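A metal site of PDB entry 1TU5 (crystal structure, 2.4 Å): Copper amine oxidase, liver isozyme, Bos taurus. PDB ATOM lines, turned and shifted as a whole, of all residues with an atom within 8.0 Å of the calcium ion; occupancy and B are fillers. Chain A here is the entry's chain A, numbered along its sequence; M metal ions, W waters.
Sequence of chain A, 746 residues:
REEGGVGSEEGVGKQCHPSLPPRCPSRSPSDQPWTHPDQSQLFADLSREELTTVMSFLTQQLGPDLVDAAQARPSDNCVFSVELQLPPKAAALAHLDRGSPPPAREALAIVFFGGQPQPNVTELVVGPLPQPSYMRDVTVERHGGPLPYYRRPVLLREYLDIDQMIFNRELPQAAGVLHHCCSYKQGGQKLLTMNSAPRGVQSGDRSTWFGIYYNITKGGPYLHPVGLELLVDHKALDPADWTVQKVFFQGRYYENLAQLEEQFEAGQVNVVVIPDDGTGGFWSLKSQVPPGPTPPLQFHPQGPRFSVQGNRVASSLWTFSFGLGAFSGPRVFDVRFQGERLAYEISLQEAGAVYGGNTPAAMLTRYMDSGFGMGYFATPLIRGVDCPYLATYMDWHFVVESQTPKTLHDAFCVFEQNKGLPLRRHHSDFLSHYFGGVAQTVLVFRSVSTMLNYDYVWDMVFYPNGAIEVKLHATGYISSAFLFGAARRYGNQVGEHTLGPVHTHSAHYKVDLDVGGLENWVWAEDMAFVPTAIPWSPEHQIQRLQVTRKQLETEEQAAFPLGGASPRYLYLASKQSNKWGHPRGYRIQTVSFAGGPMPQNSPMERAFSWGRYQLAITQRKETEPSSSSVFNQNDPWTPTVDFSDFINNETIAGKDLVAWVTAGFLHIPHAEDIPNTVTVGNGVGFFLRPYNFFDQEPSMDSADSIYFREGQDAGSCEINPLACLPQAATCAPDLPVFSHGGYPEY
The side-chain carboxylate (OE2) of Glu 650 lies within salt-bridge range of the side-chain amino group (NZ) of Lys 621.
The side-chain carboxylate of Glu 555 lies close to the backbone NH of Gln 619, at 2.9 Å.
OD1 of Asn 648 is bound to the calcium ion (2.4 Å).
OE1 of Glu 650 is bound to the calcium ion (2.4 Å).
The calcium ion is bound by the side-chain carboxylate (OE1) of Glu 555.
The calcium ion is bound by O of Phe 646 (2.5 Å).
Water W1 is bound to the calcium ion (2.6 Å).
The side-chain carboxylate (OE2) of Glu 555 is bound to the calcium ion.
Water W2 binds the calcium ion, 2.6 Å away.
Water W1 bridges O of Gln 619 and OE1 of Glu 624.
Water W2 bridges OE2 of Glu 624 and NZ of Lys 621.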
ATOM      1  N   GLU A 555     -26.605  17.734  -8.133  1.00  0.00           N
ATOM      2  CA  GLU A 555     -25.199  17.411  -7.874  1.00  0.00           C
ATOM      3  C   GLU A 555     -24.956  15.905  -7.863  1.00  0.00           C
ATOM      4  O   GLU A 555     -23.933  15.441  -8.342  1.00  0.00           O
ATOM      5  CB  GLU A 555     -24.763  18.022  -6.535  1.00  0.00           C
ATOM      6  CG  GLU A 555     -24.901  19.540  -6.450  1.00  0.00           C
ATOM      7  CD  GLU A 555     -24.367  20.154  -5.143  1.00  0.00           C
ATOM      8  OE1 GLU A 555     -24.562  19.537  -4.080  1.00  0.00           O
ATOM      9  OE2 GLU A 555     -23.782  21.257  -5.180  1.00  0.00           O
ATOM     10  N   GLU A 556     -25.892  15.150  -7.293  1.00  0.00           N
ATOM     11  CA  GLU A 556     -25.734  13.702  -7.229  1.00  0.00           C
ATOM     12  C   GLU A 556     -25.577  13.074  -8.630  1.00  0.00           C
ATOM     13  O   GLU A 556     -24.824  12.116  -8.817  1.00  0.00           O
ATOM     14  CB  GLU A 556     -26.921  13.065  -6.505  1.00  0.00           C
ATOM     15  CG  GLU A 556     -26.538  12.344  -5.198  1.00  0.00           C
ATOM     16  CD  GLU A 556     -26.199  13.281  -4.027  1.00  0.00           C
ATOM     17  OE1 GLU A 556     -25.853  12.772  -2.923  1.00  0.00           O
ATOM     18  OE2 GLU A 556     -26.289  14.524  -4.199  1.00  0.00           O
ATOM     19  N   ILE A 617     -19.535  17.993 -10.286  1.00  0.00           N
ATOM     20  CA  ILE A 617     -19.986  19.368 -10.429  1.00  0.00           C
ATOM     21  C   ILE A 617     -20.832  19.720  -9.207  1.00  0.00           C
ATOM     22  O   ILE A 617     -21.718  18.987  -8.836  1.00  0.00           O
ATOM     23  CB  ILE A 617     -20.878  19.557 -11.686  1.00  0.00           C
ATOM     24  CG1 ILE A 617     -20.287  18.827 -12.887  1.00  0.00           C
ATOM     25  CG2 ILE A 617     -20.975  21.036 -12.025  1.00  0.00           C
ATOM     26  CD1 ILE A 617     -18.892  19.235 -13.202  1.00  0.00           C
ATOM     27  N   THR A 618     -20.524  20.834  -8.566  1.00  0.00           N
ATOM     28  CA  THR A 618     -21.279  21.252  -7.395  1.00  0.00           C
ATOM     29  C   THR A 618     -21.558  22.758  -7.522  1.00  0.00           C
ATOM     30  O   THR A 618     -21.052  23.408  -8.432  1.00  0.00           O
ATOM     31  CB  THR A 618     -20.473  21.033  -6.098  1.00  0.00           C
ATOM     32  OG1 THR A 618     -19.324  21.884  -6.093  1.00  0.00           O
ATOM     33  CG2 THR A 618     -20.017  19.574  -5.999  1.00  0.00           C
ATOM     34  N   GLN A 619     -22.347  23.308  -6.619  1.00  0.00           N
ATOM     35  CA  GLN A 619     -22.577  24.752  -6.635  1.00  0.00           C
ATOM     36  C   GLN A 619     -21.343  25.423  -5.996  1.00  0.00           C
ATOM     37  O   GLN A 619     -20.868  24.973  -4.967  1.00  0.00           O
ATOM     38  CB  GLN A 619     -23.822  25.107  -5.809  1.00  0.00           C
ATOM     39  CG  GLN A 619     -25.170  25.034  -6.528  1.00  0.00           C
ATOM     40  CD  GLN A 619     -26.325  25.341  -5.589  1.00  0.00           C
ATOM     41  OE1 GLN A 619     -26.195  26.185  -4.707  1.00  0.00           O
ATOM     42  NE2 GLN A 619     -27.450  24.654  -5.770  1.00  0.00           N
ATOM     43  N   ARG A 620     -20.840  26.474  -6.630  1.00  0.00           N
ATOM     44  CA  ARG A 620     -19.684  27.248  -6.128  1.00  0.00           C
ATOM     45  C   ARG A 620     -20.174  27.842  -4.822  1.00  0.00           C
ATOM     46  O   ARG A 620     -21.204  28.475  -4.790  1.00  0.00           O
ATOM     47  CB  ARG A 620     -19.369  28.389  -7.119  1.00  0.00           C
ATOM     48  CG  ARG A 620     -18.511  29.586  -6.612  1.00  0.00           C
ATOM     49  CD  ARG A 620     -17.046  29.221  -6.569  1.00  0.00           C
ATOM     50  NE  ARG A 620     -16.071  30.310  -6.389  1.00  0.00           N
ATOM     51  CZ  ARG A 620     -16.054  31.204  -5.403  1.00  0.00           C
ATOM     52  NH1 ARG A 620     -16.985  31.233  -4.464  1.00  0.00           N
ATOM     53  NH2 ARG A 620     -15.012  32.020  -5.279  1.00  0.00           N
ATOM     54  N   LYS A 621     -19.467  27.601  -3.726  1.00  0.00           N
ATOM     55  CA  LYS A 621     -19.856  28.182  -2.452  1.00  0.00           C
ATOM     56  C   LYS A 621     -18.652  28.865  -1.822  1.00  0.00           C
ATOM     57  O   LYS A 621     -17.529  28.310  -1.812  1.00  0.00           O
ATOM     58  CB  LYS A 621     -20.388  27.119  -1.487  1.00  0.00           C
ATOM     59  CG  LYS A 621     -21.863  26.886  -1.601  1.00  0.00           C
ATOM     60  CD  LYS A 621     -22.361  25.748  -0.732  1.00  0.00           C
ATOM     61  CE  LYS A 621     -23.861  25.534  -0.959  1.00  0.00           C
ATOM     62  NZ  LYS A 621     -24.455  24.388  -0.146  1.00  0.00           N
ATOM     63  N   GLU A 624     -16.947  26.753   0.573  1.00  0.00           N
ATOM     64  CA  GLU A 624     -16.287  25.547   0.105  1.00  0.00           C
ATOM     65  C   GLU A 624     -15.173  25.935  -0.863  1.00  0.00           C
ATOM     66  O   GLU A 624     -15.214  25.572  -2.048  1.00  0.00           O
ATOM     67  CB  GLU A 624     -17.299  24.651  -0.620  1.00  0.00           C
ATOM     68  CG  GLU A 624     -18.407  24.148   0.269  1.00  0.00           C
ATOM     69  CD  GLU A 624     -19.520  23.502  -0.506  1.00  0.00           C
ATOM     70  OE1 GLU A 624     -19.479  23.549  -1.752  1.00  0.00           O
ATOM     71  OE2 GLU A 624     -20.437  22.937   0.136  1.00  0.00           O
ATOM     72  N   PHE A 643     -14.367  16.375   1.014  1.00  0.00           N
ATOM     73  CA  PHE A 643     -14.948  16.795  -0.234  1.00  0.00           C
ATOM     74  C   PHE A 643     -16.353  16.253  -0.527  1.00  0.00           C
ATOM     75  O   PHE A 643     -17.212  17.005  -1.011  1.00  0.00           O
ATOM     76  CB  PHE A 643     -14.016  16.437  -1.412  1.00  0.00           C
ATOM     77  CG  PHE A 643     -14.585  16.801  -2.747  1.00  0.00           C
ATOM     78  CD1 PHE A 643     -14.673  18.120  -3.146  1.00  0.00           C
ATOM     79  CD2 PHE A 643     -15.084  15.824  -3.601  1.00  0.00           C
ATOM     80  CE1 PHE A 643     -15.257  18.458  -4.378  1.00  0.00           C
ATOM     81  CE2 PHE A 643     -15.662  16.164  -4.807  1.00  0.00           C
ATOM     82  CZ  PHE A 643     -15.757  17.465  -5.195  1.00  0.00           C
ATOM     83  N   SER A 644     -16.609  14.974  -0.234  1.00  0.00           N
ATOM     84  CA  SER A 644     -17.945  14.438  -0.537  1.00  0.00           C
ATOM     85  C   SER A 644     -19.045  15.218   0.174  1.00  0.00           C
ATOM     86  O   SER A 644     -20.197  15.217  -0.273  1.00  0.00           O
ATOM     87  CB  SER A 644     -18.046  12.954  -0.205  1.00  0.00           C
ATOM     88  OG  SER A 644     -17.699  12.733   1.135  1.00  0.00           O
ATOM     89  N   ASP A 645     -18.694  15.900   1.256  1.00  0.00           N
ATOM     90  CA  ASP A 645     -19.678  16.710   1.956  1.00  0.00           C
ATOM     91  C   ASP A 645     -20.257  17.751   1.013  1.00  0.00           C
ATOM     92  O   ASP A 645     -21.399  18.166   1.198  1.00  0.00           O
ATOM     93  CB  ASP A 645     -19.046  17.453   3.145  1.00  0.00           C
ATOM     94  CG  ASP A 645     -18.814  16.560   4.360  1.00  0.00           C
ATOM     95  OD1 ASP A 645     -18.093  16.999   5.291  1.00  0.00           O
ATOM     96  OD2 ASP A 645     -19.343  15.431   4.400  1.00  0.00           O
ATOM     97  N   PHE A 646     -19.472  18.194   0.036  1.00  0.00           N
ATOM     98  CA  PHE A 646     -19.950  19.211  -0.908  1.00  0.00           C
ATOM     99  C   PHE A 646     -21.048  18.695  -1.824  1.00  0.00           C
ATOM    100  O   PHE A 646     -21.787  19.480  -2.415  1.00  0.00           O
ATOM    101  CB  PHE A 646     -18.822  19.729  -1.796  1.00  0.00           C
ATOM    102  CG  PHE A 646     -17.687  20.360  -1.041  1.00  0.00           C
ATOM    103  CD1 PHE A 646     -17.711  20.470   0.340  1.00  0.00           C
ATOM    104  CD2 PHE A 646     -16.568  20.823  -1.724  1.00  0.00           C
ATOM    105  CE1 PHE A 646     -16.642  21.044   1.023  1.00  0.00           C
ATOM    106  CE2 PHE A 646     -15.486  21.395  -1.029  1.00  0.00           C
ATOM    107  CZ  PHE A 646     -15.529  21.495   0.343  1.00  0.00           C
ATOM    108  N   ILE A 647     -21.147  17.375  -1.941  1.00  0.00           N
ATOM    109  CA  ILE A 647     -22.150  16.761  -2.813  1.00  0.00           C
ATOM    110  C   ILE A 647     -23.368  16.400  -1.975  1.00  0.00           C
ATOM    111  O   ILE A 647     -23.404  15.329  -1.349  1.00  0.00           O
ATOM    112  CB  ILE A 647     -21.552  15.514  -3.489  1.00  0.00           C
ATOM    113  CG1 ILE A 647     -20.294  15.914  -4.281  1.00  0.00           C
ATOM    114  CG2 ILE A 647     -22.562  14.895  -4.439  1.00  0.00           C
ATOM    115  CD1 ILE A 647     -19.430  14.741  -4.674  1.00  0.00           C
ATOM    116  N   ASN A 648     -24.351  17.286  -1.957  1.00  0.00           N
ATOM    117  CA  ASN A 648     -25.558  17.072  -1.152  1.00  0.00           C
ATOM    118  C   ASN A 648     -26.881  17.291  -1.862  1.00  0.00           C
ATOM    119  O   ASN A 648     -27.769  17.957  -1.334  1.00  0.00           O
ATOM    120  CB  ASN A 648     -25.487  17.932   0.124  1.00  0.00           C
ATOM    121  CG  ASN A 648     -25.534  19.436  -0.142  1.00  0.00           C
ATOM    122  OD1 ASN A 648     -24.799  19.976  -0.998  1.00  0.00           O
ATOM    123  ND2 ASN A 648     -26.382  20.138   0.599  1.00  0.00           N
ATOM    124  N   ASN A 649     -26.993  16.721  -3.053  1.00  0.00           N
ATOM    125  CA  ASN A 649     -28.213  16.783  -3.869  1.00  0.00           C
ATOM    126  C   ASN A 649     -28.826  18.169  -4.163  1.00  0.00           C
ATOM    127  O   ASN A 649     -30.030  18.259  -4.370  1.00  0.00           O
ATOM    128  CB  ASN A 649     -29.275  15.887  -3.232  1.00  0.00           C
ATOM    129  CG  ASN A 649     -30.017  15.017  -4.256  1.00  0.00           C
ATOM    130  OD1 ASN A 649     -30.061  15.345  -5.442  1.00  0.00           O
ATOM    131  ND2 ASN A 649     -30.601  13.919  -3.787  1.00  0.00           N
ATOM    132  N   GLU A 650     -28.026  19.222  -4.192  1.00  0.00           N
ATOM    133  CA  GLU A 650     -28.571  20.542  -4.496  1.00  0.00           C
ATOM    134  C   GLU A 650     -28.809  20.667  -6.009  1.00  0.00           C
ATOM    135  O   GLU A 650     -28.330  19.864  -6.801  1.00  0.00           O
ATOM    136  CB  GLU A 650     -27.618  21.654  -4.034  1.00  0.00           C
ATOM    137  CG  GLU A 650     -27.398  21.684  -2.539  1.00  0.00           C
ATOM    138  CD  GLU A 650     -26.490  22.840  -2.078  1.00  0.00           C
ATOM    139  OE1 GLU A 650     -25.335  22.962  -2.575  1.00  0.00           O
ATOM    140  OE2 GLU A 650     -26.914  23.629  -1.203  1.00  0.00           O
ATOM    141  N   THR A 651     -29.557  21.677  -6.422  1.00  0.00           N
ATOM    142  CA  THR A 651     -29.812  21.839  -7.839  1.00  0.00           C
ATOM    143  C   THR A 651     -28.551  22.321  -8.538  1.00  0.00           C
ATOM    144  O   THR A 651     -27.719  23.012  -7.967  1.00  0.00           O
ATOM    145  CB  THR A 651     -30.929  22.880  -8.125  1.00  0.00           C
ATOM    146  OG1 THR A 651     -31.065  23.056  -9.551  1.00  0.00           O
ATOM    147  CG2 THR A 651     -30.604  24.232  -7.489  1.00  0.00           C
ATOM    148  N   ILE A 652     -28.375  21.939  -9.792  1.00  0.00           N
ATOM    149  CA  ILE A 652     -27.236  22.436 -10.571  1.00  0.00           C
ATOM    150  C   ILE A 652     -27.806  22.989 -11.872  1.00  0.00           C
ATOM    151  O   ILE A 652     -27.153  22.971 -12.917  1.00  0.00           O
ATOM    152  CB  ILE A 652     -26.152  21.359 -10.852  1.00  0.00           C
ATOM    153  CG1 ILE A 652     -26.746  20.188 -11.635  1.00  0.00           C
ATOM    154  CG2 ILE A 652     -25.536  20.897  -9.543  1.00  0.00           C
ATOM    155  CD1 ILE A 652     -25.699  19.123 -12.011  1.00  0.00           C
HETATM  156 CA    CA M   1     -23.566  21.290  -2.607  1.00  0.00          CA
HETATM  157  O   HOH W   1     -21.820  23.063  -3.240  1.00  0.00           O
HETATM  158  O   HOH W   2     -22.904  21.860  -0.127  1.00  0.00           O
